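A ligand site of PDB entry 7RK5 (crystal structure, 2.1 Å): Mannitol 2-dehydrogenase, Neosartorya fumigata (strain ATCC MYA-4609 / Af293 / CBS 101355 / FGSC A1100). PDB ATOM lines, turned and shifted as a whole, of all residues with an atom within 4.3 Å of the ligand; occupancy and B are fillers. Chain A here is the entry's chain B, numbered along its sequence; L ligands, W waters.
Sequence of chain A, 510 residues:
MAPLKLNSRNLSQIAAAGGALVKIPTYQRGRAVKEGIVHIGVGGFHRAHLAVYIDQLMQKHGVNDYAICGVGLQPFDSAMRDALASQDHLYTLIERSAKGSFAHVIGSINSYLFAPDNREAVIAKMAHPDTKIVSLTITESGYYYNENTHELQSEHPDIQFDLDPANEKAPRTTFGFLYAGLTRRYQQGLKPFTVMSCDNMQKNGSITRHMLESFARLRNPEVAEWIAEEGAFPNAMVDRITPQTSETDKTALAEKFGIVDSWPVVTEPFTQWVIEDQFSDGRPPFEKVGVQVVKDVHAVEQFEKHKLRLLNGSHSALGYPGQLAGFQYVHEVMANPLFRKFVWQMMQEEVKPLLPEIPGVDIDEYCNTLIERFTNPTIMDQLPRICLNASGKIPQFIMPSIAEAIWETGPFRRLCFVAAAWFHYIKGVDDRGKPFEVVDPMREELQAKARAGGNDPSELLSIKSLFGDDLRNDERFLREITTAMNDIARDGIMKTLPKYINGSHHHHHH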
ATOM      1  N   GLY A  41      -2.001  -6.861 -11.249  1.00  0.00           N
ATOM      2  CA  GLY A  41      -3.361  -7.217 -10.937  1.00  0.00           C
ATOM      3  C   GLY A  41      -3.484  -7.805  -9.553  1.00  0.00           C
ATOM      4  O   GLY A  41      -3.783  -9.002  -9.408  1.00  0.00           O
ATOM      5  N   VAL A  42      -3.266  -6.990  -8.516  1.00  0.00           N
ATOM      6  CA  VAL A  42      -3.404  -7.452  -7.125  1.00  0.00           C
ATOM      7  C   VAL A  42      -4.891  -7.416  -6.780  1.00  0.00           C
ATOM      8  O   VAL A  42      -5.476  -6.355  -6.582  1.00  0.00           O
ATOM      9  CB  VAL A  42      -2.573  -6.607  -6.156  1.00  0.00           C
ATOM     10  CG1 VAL A  42      -2.787  -7.079  -4.709  1.00  0.00           C
ATOM     11  CG2 VAL A  42      -1.099  -6.680  -6.533  1.00  0.00           C
ATOM     12  N   GLY A  43      -5.504  -8.599  -6.740  1.00  0.00           N
ATOM     13  CA  GLY A  43      -6.884  -8.801  -6.353  1.00  0.00           C
ATOM     14  C   GLY A  43      -6.972  -9.854  -5.262  1.00  0.00           C
ATOM     15  O   GLY A  43      -6.040 -10.064  -4.477  1.00  0.00           O
ATOM     16  N   GLY A  44      -8.113 -10.545  -5.229  1.00  0.00           N
ATOM     17  CA  GLY A  44      -8.322 -11.534  -4.176  1.00  0.00           C
ATOM     18  C   GLY A  44      -7.456 -12.758  -4.383  1.00  0.00           C
ATOM     19  O   GLY A  44      -6.756 -13.203  -3.461  1.00  0.00           O
ATOM     20  N   PHE A  45      -7.477 -13.312  -5.590  1.00  0.00           N
ATOM     21  CA  PHE A  45      -6.828 -14.593  -5.817  1.00  0.00           C
ATOM     22  C   PHE A  45      -5.318 -14.482  -5.669  1.00  0.00           C
ATOM     23  O   PHE A  45      -4.700 -15.350  -5.040  1.00  0.00           O
ATOM     24  CB  PHE A  45      -7.208 -15.170  -7.179  1.00  0.00           C
ATOM     25  CG  PHE A  45      -6.599 -16.525  -7.429  1.00  0.00           C
ATOM     26  CD1 PHE A  45      -7.074 -17.650  -6.746  1.00  0.00           C
ATOM     27  CD2 PHE A  45      -5.541 -16.679  -8.313  1.00  0.00           C
ATOM     28  CE1 PHE A  45      -6.486 -18.908  -6.944  1.00  0.00           C
ATOM     29  CE2 PHE A  45      -4.957 -17.929  -8.521  1.00  0.00           C
ATOM     30  CZ  PHE A  45      -5.431 -19.049  -7.817  1.00  0.00           C
ATOM     31  N   LEU A  73      -2.963  -1.712 -12.761  1.00  0.00           N
ATOM     32  CA  LEU A  73      -3.113  -0.995 -14.017  1.00  0.00           C
ATOM     33  C   LEU A  73      -4.514  -0.441 -14.233  1.00  0.00           C
ATOM     34  O   LEU A  73      -4.657   0.529 -14.983  1.00  0.00           O
ATOM     35  CB  LEU A  73      -2.778  -1.918 -15.202  1.00  0.00           C
ATOM     36  CG  LEU A  73      -1.344  -2.051 -15.720  1.00  0.00           C
ATOM     37  CD1 LEU A  73      -0.341  -2.105 -14.598  1.00  0.00           C
ATOM     38  CD2 LEU A  73      -1.268  -3.291 -16.564  1.00  0.00           C
ATOM     39  N   GLN A  74      -5.537  -1.039 -13.634  1.00  0.00           N
ATOM     40  CA  GLN A  74      -6.919  -0.615 -13.825  1.00  0.00           C
ATOM     41  C   GLN A  74      -7.268   0.523 -12.869  1.00  0.00           C
ATOM     42  O   GLN A  74      -6.739   0.592 -11.762  1.00  0.00           O
ATOM     43  CB  GLN A  74      -7.876  -1.767 -13.577  1.00  0.00           C
ATOM     44  CG  GLN A  74      -7.624  -2.936 -14.486  1.00  0.00           C
ATOM     45  CD  GLN A  74      -7.815  -2.567 -15.920  1.00  0.00           C
ATOM     46  OE1 GLN A  74      -8.943  -2.485 -16.409  1.00  0.00           O
ATOM     47  NE2 GLN A  74      -6.713  -2.297 -16.607  1.00  0.00           N
ATOM     48  N   ASP A  77      -7.816  -0.291  -9.259  1.00  0.00           N
ATOM     49  CA  ASP A  77      -6.663  -0.684  -8.460  1.00  0.00           C
ATOM     50  C   ASP A  77      -6.167   0.418  -7.538  1.00  0.00           C
ATOM     51  O   ASP A  77      -5.290   0.143  -6.700  1.00  0.00           O
ATOM     52  CB  ASP A  77      -5.506  -1.107  -9.349  1.00  0.00           C
ATOM     53  CG  ASP A  77      -5.804  -2.364 -10.109  1.00  0.00           C
ATOM     54  OD1 ASP A  77      -6.448  -3.262  -9.538  1.00  0.00           O
ATOM     55  OD2 ASP A  77      -5.388  -2.456 -11.286  1.00  0.00           O
ATOM     56  N   THR A 137      -2.455 -11.755 -12.521  1.00  0.00           N
ATOM     57  CA  THR A 137      -3.876 -12.109 -12.396  1.00  0.00           C
ATOM     58  C   THR A 137      -4.601 -10.913 -12.991  1.00  0.00           C
ATOM     59  O   THR A 137      -4.941  -9.967 -12.271  1.00  0.00           O
ATOM     60  CB  THR A 137      -4.347 -12.400 -10.943  1.00  0.00           C
ATOM     61  OG1 THR A 137      -3.929 -11.352 -10.061  1.00  0.00           O
ATOM     62  CG2 THR A 137      -3.848 -13.788 -10.418  1.00  0.00           C
ATOM     63  N   ILE A 138      -4.823 -10.935 -14.301  1.00  0.00           N
ATOM     64  CA  ILE A 138      -5.409  -9.813 -15.019  1.00  0.00           C
ATOM     65  C   ILE A 138      -6.732 -10.176 -15.676  1.00  0.00           C
ATOM     66  O   ILE A 138      -7.258  -9.396 -16.467  1.00  0.00           O
ATOM     67  CB  ILE A 138      -4.420  -9.256 -16.066  1.00  0.00           C
ATOM     68  CG1 ILE A 138      -4.131 -10.301 -17.134  1.00  0.00           C
ATOM     69  CG2 ILE A 138      -3.124  -8.841 -15.415  1.00  0.00           C
ATOM     70  CD1 ILE A 138      -3.173  -9.830 -18.206  1.00  0.00           C
ATOM     71  N   THR A 139      -7.295 -11.350 -15.365  1.00  0.00           N
ATOM     72  CA  THR A 139      -8.519 -11.864 -15.968  1.00  0.00           C
ATOM     73  C   THR A 139      -8.328 -12.134 -17.461  1.00  0.00           C
ATOM     74  O   THR A 139      -7.440 -11.575 -18.106  1.00  0.00           O
ATOM     75  CB  THR A 139      -9.718 -10.917 -15.756  1.00  0.00           C
ATOM     76  OG1 THR A 139      -9.604  -9.784 -16.632  1.00  0.00           O
ATOM     77  CG2 THR A 139      -9.826 -10.442 -14.277  1.00  0.00           C
ATOM     78  N   GLY A 142      -7.810  -9.287 -19.914  1.00  0.00           N
ATOM     79  CA  GLY A 142      -6.565  -8.548 -19.920  1.00  0.00           C
ATOM     80  C   GLY A 142      -5.515  -9.035 -20.901  1.00  0.00           C
ATOM     81  O   GLY A 142      -4.515  -8.339 -21.099  1.00  0.00           O
ATOM     82  N   THR A 174      -0.959  -4.496 -20.035  1.00  0.00           N
ATOM     83  CA  THR A 174       0.050  -5.360 -19.451  1.00  0.00           C
ATOM     84  C   THR A 174       1.234  -5.539 -20.389  1.00  0.00           C
ATOM     85  O   THR A 174       2.404  -5.415 -19.973  1.00  0.00           O
ATOM     86  CB  THR A 174      -0.576  -6.723 -19.093  1.00  0.00           C
ATOM     87  OG1 THR A 174      -1.521  -6.550 -18.043  1.00  0.00           O
ATOM     88  CG2 THR A 174       0.495  -7.708 -18.647  1.00  0.00           C
ATOM     89  N   CYS A 198      -1.099 -16.314 -13.668  1.00  0.00           N
ATOM     90  CA  CYS A 198      -1.866 -17.071 -12.684  1.00  0.00           C
ATOM     91  C   CYS A 198      -3.367 -16.987 -12.919  1.00  0.00           C
ATOM     92  O   CYS A 198      -4.157 -17.188 -11.990  1.00  0.00           O
ATOM     93  CB  CYS A 198      -1.533 -16.627 -11.247  1.00  0.00           C
ATOM     94  SG  CYS A 198       0.249 -16.708 -10.890  1.00  0.00           S
ATOM     95  N   ASP A 199      -3.794 -16.723 -14.145  1.00  0.00           N
ATOM     96  CA  ASP A 199      -5.205 -16.760 -14.467  1.00  0.00           C
ATOM     97  C   ASP A 199      -5.638 -18.182 -14.843  1.00  0.00           C
ATOM     98  O   ASP A 199      -4.815 -19.040 -15.176  1.00  0.00           O
ATOM     99  CB  ASP A 199      -5.504 -15.758 -15.576  1.00  0.00           C
ATOM    100  CG  ASP A 199      -5.382 -14.314 -15.101  1.00  0.00           C
ATOM    101  OD1 ASP A 199      -6.275 -13.877 -14.350  1.00  0.00           O
ATOM    102  OD2 ASP A 199      -4.383 -13.643 -15.445  1.00  0.00           O
ATOM    103  N   ASN A 200      -6.960 -18.438 -14.790  1.00  0.00           N
ATOM    104  CA  ASN A 200      -7.528 -19.785 -14.815  1.00  0.00           C
ATOM    105  C   ASN A 200      -7.801 -20.313 -16.234  1.00  0.00           C
ATOM    106  O   ASN A 200      -8.466 -21.339 -16.381  1.00  0.00           O
ATOM    107  CB  ASN A 200      -8.829 -19.818 -13.992  1.00  0.00           C
ATOM    108  CG  ASN A 200      -9.323 -21.247 -13.684  1.00  0.00           C
ATOM    109  OD1 ASN A 200      -8.547 -22.112 -13.283  1.00  0.00           O
ATOM    110  ND2 ASN A 200     -10.622 -21.492 -13.878  1.00  0.00           N
ATOM    111  N   VAL A 238      -3.977 -23.305 -11.255  1.00  0.00           N
ATOM    112  CA  VAL A 238      -4.084 -22.600  -9.982  1.00  0.00           C
ATOM    113  C   VAL A 238      -5.466 -22.864  -9.419  1.00  0.00           C
ATOM    114  O   VAL A 238      -6.465 -22.882 -10.147  1.00  0.00           O
ATOM    115  CB  VAL A 238      -3.813 -21.083 -10.136  1.00  0.00           C
ATOM    116  CG1 VAL A 238      -2.344 -20.828 -10.572  1.00  0.00           C
ATOM    117  CG2 VAL A 238      -4.787 -20.431 -11.119  1.00  0.00           C
ATOM    118  N   ARG A 240      -7.698 -22.061  -5.707  1.00  0.00           N
ATOM    119  CA  ARG A 240      -8.085 -21.710  -4.340  1.00  0.00           C
ATOM    120  C   ARG A 240      -9.323 -20.806  -4.364  1.00  0.00           C
ATOM    121  O   ARG A 240      -9.281 -19.718  -4.938  1.00  0.00           O
ATOM    122  CB  ARG A 240      -6.939 -21.009  -3.589  1.00  0.00           C
ATOM    123  CG  ARG A 240      -7.302 -20.701  -2.134  1.00  0.00           C
ATOM    124  CD  ARG A 240      -6.127 -20.136  -1.293  1.00  0.00           C
ATOM    125  NE  ARG A 240      -6.352 -20.386   0.130  1.00  0.00           N
ATOM    126  CZ  ARG A 240      -5.398 -20.400   1.052  1.00  0.00           C
ATOM    127  NH1 ARG A 240      -4.140 -20.157   0.701  1.00  0.00           N
ATOM    128  NH2 ARG A 240      -5.683 -20.684   2.306  1.00  0.00           N
ATOM    129  N   ILE A 241     -10.430 -21.252  -3.770  1.00  0.00           N
ATOM    130  CA  ILE A 241     -11.677 -20.502  -3.923  1.00  0.00           C
ATOM    131  C   ILE A 241     -11.602 -19.241  -3.063  1.00  0.00           C
ATOM    132  O   ILE A 241     -11.413 -19.310  -1.846  1.00  0.00           O
ATOM    133  CB  ILE A 241     -12.892 -21.365  -3.562  1.00  0.00           C
ATOM    134  CG1 ILE A 241     -13.070 -22.510  -4.583  1.00  0.00           C
ATOM    135  CG2 ILE A 241     -14.154 -20.539  -3.535  1.00  0.00           C
ATOM    136  CD1 ILE A 241     -13.700 -23.770  -4.010  1.00  0.00           C
ATOM    137  N   THR A 242     -11.751 -18.079  -3.706  1.00  0.00           N
ATOM    138  CA  THR A 242     -11.536 -16.765  -3.085  1.00  0.00           C
ATOM    139  C   THR A 242     -12.698 -15.846  -3.456  1.00  0.00           C
ATOM    140  O   THR A 242     -12.648 -15.153  -4.470  1.00  0.00           O
ATOM    141  CB  THR A 242     -10.209 -16.161  -3.541  1.00  0.00           C
ATOM    142  OG1 THR A 242      -9.168 -17.125  -3.407  1.00  0.00           O
ATOM    143  CG2 THR A 242      -9.853 -14.959  -2.687  1.00  0.00           C
ATOM    144  N   GLN A 244     -15.246 -12.478  -2.966  1.00  0.00           N
ATOM    145  CA  GLN A 244     -15.019 -11.077  -2.669  1.00  0.00           C
ATOM    146  C   GLN A 244     -15.308 -10.792  -1.193  1.00  0.00           C
ATOM    147  O   GLN A 244     -16.097 -11.482  -0.545  1.00  0.00           O
ATOM    148  CB  GLN A 244     -15.905 -10.188  -3.535  1.00  0.00           C
ATOM    149  CG  GLN A 244     -15.316  -9.905  -4.889  1.00  0.00           C
ATOM    150  CD  GLN A 244     -15.390 -11.105  -5.796  1.00  0.00           C
ATOM    151  OE1 GLN A 244     -14.404 -11.843  -5.952  1.00  0.00           O
ATOM    152  NE2 GLN A 244     -16.553 -11.312  -6.386  1.00  0.00           N
ATOM    153  N   LYS A 307      -9.450 -29.559 -13.401  1.00  0.00           N
ATOM    154  CA  LYS A 307     -10.032 -28.475 -12.630  1.00  0.00           C
ATOM    155  C   LYS A 307     -11.208 -27.827 -13.360  1.00  0.00           C
ATOM    156  O   LYS A 307     -12.301 -27.662 -12.794  1.00  0.00           O
ATOM    157  CB  LYS A 307      -8.959 -27.438 -12.318  1.00  0.00           C
ATOM    158  CG  LYS A 307      -9.419 -26.435 -11.275  1.00  0.00           C
ATOM    159  CD  LYS A 307      -9.009 -25.029 -11.625  1.00  0.00           C
ATOM    160  CE  LYS A 307      -9.667 -24.062 -10.639  1.00  0.00           C
ATOM    161  NZ  LYS A 307      -9.325 -22.664 -10.962  1.00  0.00           N
ATOM    162  N   ARG A 385     -22.263 -14.881  -7.230  1.00  0.00           N
ATOM    163  CA  ARG A 385     -20.863 -14.780  -7.645  1.00  0.00           C
ATOM    164  C   ARG A 385     -20.482 -15.916  -8.585  1.00  0.00           C
ATOM    165  O   ARG A 385     -19.732 -15.710  -9.550  1.00  0.00           O
ATOM    166  CB  ARG A 385     -19.930 -14.786  -6.435  1.00  0.00           C
ATOM    167  CG  ARG A 385     -18.434 -14.634  -6.774  1.00  0.00           C
ATOM    168  CD  ARG A 385     -17.491 -14.816  -5.560  1.00  0.00           C
ATOM    169  NE  ARG A 385     -17.239 -16.232  -5.298  1.00  0.00           N
ATOM    170  CZ  ARG A 385     -16.322 -16.953  -5.929  1.00  0.00           C
ATOM    171  NH1 ARG A 385     -15.555 -16.388  -6.855  1.00  0.00           N
ATOM    172  NH2 ARG A 385     -16.174 -18.253  -5.654  1.00  0.00           N
HETATM  173  P1  LIG L   1     -10.343  -9.411  -8.582  1.00  0.00           P
HETATM  174  O1  LIG L   1     -10.156  -9.465  -7.087  1.00  0.00           O
HETATM  175  O2  LIG L   1     -11.549  -8.672  -8.987  1.00  0.00           O
HETATM  176  O3  LIG L   1      -9.049  -8.706  -9.235  1.00  0.00           O
HETATM  177  C1  LIG L   1      -8.633  -9.048 -10.551  1.00  0.00           C
HETATM  178  C2  LIG L   1      -7.457  -8.108 -10.997  1.00  0.00           C
HETATM  179  O4  LIG L   1      -7.530  -8.025 -12.328  1.00  0.00           O
HETATM  180  C3  LIG L   1      -7.629  -6.566 -10.399  1.00  0.00           C
HETATM  181  O5  LIG L   1      -6.342  -6.065  -9.957  1.00  0.00           O
HETATM  182  C4  LIG L   1      -8.036  -5.852 -11.419  1.00  0.00           C
HETATM  183  O6  LIG L   1      -7.615  -4.497 -11.372  1.00  0.00           O
HETATM  184  C5  LIG L   1      -7.261  -6.547 -12.602  1.00  0.00           C
HETATM  185  N1  LIG L   1      -7.614  -6.424 -14.005  1.00  0.00           N
HETATM  186  C6  LIG L   1      -8.823  -6.604 -14.540  1.00  0.00           C
HETATM  187  N2  LIG L   1      -8.737  -6.376 -15.847  1.00  0.00           N
HETATM  188  C7  LIG L   1      -7.485  -6.017 -16.146  1.00  0.00           C
HETATM  189  C8  LIG L   1      -6.768  -5.653 -17.285  1.00  0.00           C
HETATM  190  N3  LIG L   1      -7.450  -5.599 -18.585  1.00  0.00           N
HETATM  191  N4  LIG L   1      -5.503  -5.363 -17.220  1.00  0.00           N
HETATM  192  C9  LIG L   1      -4.853  -5.405 -16.054  1.00  0.00           C
HETATM  193  N5  LIG L   1      -5.473  -5.732 -14.942  1.00  0.00           N
HETATM  194  C10 LIG L   1      -6.768  -6.060 -14.961  1.00  0.00           C
HETATM  195  O7  LIG L   1     -10.564 -10.939  -9.148  1.00  0.00           O
HETATM  196  P2  LIG L   1      -9.796 -12.332  -8.586  1.00  0.00           P
HETATM  197  O8  LIG L   1     -10.746 -13.116  -7.657  1.00  0.00           O
HETATM  198  O9  LIG L   1      -8.481 -12.004  -7.906  1.00  0.00           O
HETATM  199  O10 LIG L   1      -9.468 -13.252  -9.896  1.00  0.00           O
HETATM  200  C11 LIG L   1      -8.874 -12.641 -11.001  1.00  0.00           C
HETATM  201  C12 LIG L   1      -8.060 -13.753 -11.710  1.00  0.00           C
HETATM  202  O11 LIG L   1      -7.709 -14.650 -10.788  1.00  0.00           O
HETATM  203  C13 LIG L   1      -8.958 -14.530 -12.770  1.00  0.00           C
HETATM  204  O12 LIG L   1     -10.245 -13.962 -12.926  1.00  0.00           O
HETATM  205  C14 LIG L   1      -9.099 -15.975 -12.215  1.00  0.00           C
HETATM  206  O13 LIG L   1      -8.860 -16.782 -13.346  1.00  0.00           O
HETATM  207  C15 LIG L   1      -8.093 -16.142 -11.306  1.00  0.00           C
HETATM  208  N6  LIG L   1      -8.636 -17.056 -10.289  1.00  0.00           N
HETATM  209  C16 LIG L   1      -9.570 -16.570  -9.304  1.00  0.00           C
HETATM  210  C17 LIG L   1     -10.239 -17.554  -8.412  1.00  0.00           C
HETATM  211  C18 LIG L   1     -11.156 -17.052  -7.312  1.00  0.00           C
HETATM  212  O14 LIG L   1     -11.284 -15.870  -7.124  1.00  0.00           O
HETATM  213  N7  LIG L   1     -11.871 -18.076  -6.515  1.00  0.00           N
HETATM  214  C19 LIG L   1     -10.061 -19.068  -8.543  1.00  0.00           C
HETATM  215  C20 LIG L   1      -8.782 -19.413  -9.318  1.00  0.00           C
HETATM  216  C21 LIG L   1      -8.233 -18.407 -10.297  1.00  0.00           C
HETATM  217  O   HOH W   1     -12.717  -9.543 -11.329  1.00  0.00           O
HETATM  218  O   HOH W   2     -11.831 -21.093 -10.637  1.00  0.00           O
HETATM  219  O   HOH W   3     -11.682 -11.926  -5.016  1.00  0.00           O
HETATM  220  O   HOH W   4      -4.186  -4.357 -12.690  1.00  0.00           O
HETATM  221  O   HOH W   5     -10.171 -22.133  -7.761  1.00  0.00           O
HETATM  222  O   HOH W   6      -9.945  -7.506  -5.366  1.00  0.00           O
HETATM  223  O   HOH W   7      -4.330  -4.403  -7.733  1.00  0.00           O
HETATM  224  O   HOH W   8      -5.637 -11.276  -7.896  1.00  0.00           O
HETATM  225  O   HOH W   9     -11.444  -6.551 -16.778  1.00  0.00           O
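Water W4 lies within hydrogen-bond range of OD2 of Asp 77 (2.7 Å), N of Leu 73 (2.9 Å) and N5 of the ligand (2.9 Å).
Water W8 lies within hydrogen-bond range of the side-chain hydroxyl of Thr 137, the backbone NH of Gly 43, an oxygen (O9) of the ligand and the backbone carbonyl oxygen of Gly 41.
Water W3 lies within hydrogen-bond range of the side-chain amide oxygen of Gln 244 (2.9 Å), an oxygen (O8) of the ligand (3.0 Å) and the backbone carbonyl oxygen of Thr 242 (3.4 Å).
Water W5 bridges N of Arg 240 (3.2 Å) and NZ of Lys 307 (3.4 Å).
Water W2 bridges NZ of Lys 307 and ND2 of Asn 200.
Water W7 lies within hydrogen-bond range of the backbone carbonyl oxygen of Val 42 (2.5 Å), the side-chain carboxylate of Asp 77 (3.0 Å) and an oxygen (O5) of the ligand (3.4 Å).
The side-chain carboxylate (OD2) of Asp 77 sits at hydrogen-bond distance from the backbone NH (N) of Gln 74, 2.7 Å away.
The side-chain carboxylate (OD2) of Asp 77 lies within hydrogen-bond range of the backbone NH (N) of Leu 73 (2.9 Å).
The side-chain hydroxyl of Thr 242 lies within hydrogen-bond range of the backbone carbonyl oxygen of Arg 240.
NZ of Lys 307 lies within hydrogen-bond range of OD1 of Asn 200 (2.5 Å).
N of Ile 138 lies within hydrogen-bond range of OD2 of Asp 199.
The side-chain carboxylate (OD1) of Asp 199 lies within hydrogen-bond range of the backbone NH (N) of Thr 139 (2.9 Å).
O of Gly 41 lies within hydrogen-bond range of OG1 of Thr 137.
The side-chain amino group of Lys 307 sits at hydrogen-bond distance from the backbone carbonyl oxygen of Val 238, 3.0 Å away.
OD1 of Asp 77 sits at hydrogen-bond distance from O6 of the ligand.
O9 of the ligand is in hydrogen-bond range of N of Phe 45 (2.8 Å).
N of Asn 200 lies within hydrogen-bond range of O13 of the ligand (2.9 Å).
An oxygen (O1) of the ligand is in hydrogen-bond range of the backbone NH (N) of Gly 44 (3.0 Å).
NE2 of Gln 74 sits at hydrogen-bond distance from N4 of the ligand.
The backbone carbonyl oxygen of Arg 240 is in hydrogen-bond range of a nitrogen (N7) of the ligand, 3.4 Å away.
O5 of the ligand is in hydrogen-bond range of O of Val 42, at 3.5 Å.
An oxygen (O4) of the ligand lies close to the backbone carbonyl oxygen (O) of Thr 137, 3.2 Å away.
A nitrogen (N2) of the ligand sits close to the backbone carbonyl oxygen of Ile 138, at 3.4 Å.
N7 of the ligand sits close to N of Thr 242 (2.8 Å).
Gly 41 touches the ligand.
CA of Gly 43 touches O1 of the ligand, at 3.4 Å.
Thr 139 touches the ligand (OG1 to N2, 3.6 Å).
CA of Gly 142 touches N3 of the ligand (3.4 Å).
Asp 199 touches the ligand (OD1 to C13, 3.2 Å).
CA of Ile 241 touches N7 of the ligand, at 3.6 Å.
Lys 307 touches the ligand.
17 residues have an atom within 4 Å of the ligand: Gly 41, Val 42, Gly 43, Gly 44, Phe 45, Gln 74, Asp 77, Thr 137, Ile 138, Thr 139, Gly 142, Asp 199, Asn 200, Arg 240, Ile 241, Thr 242 and Lys 307.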
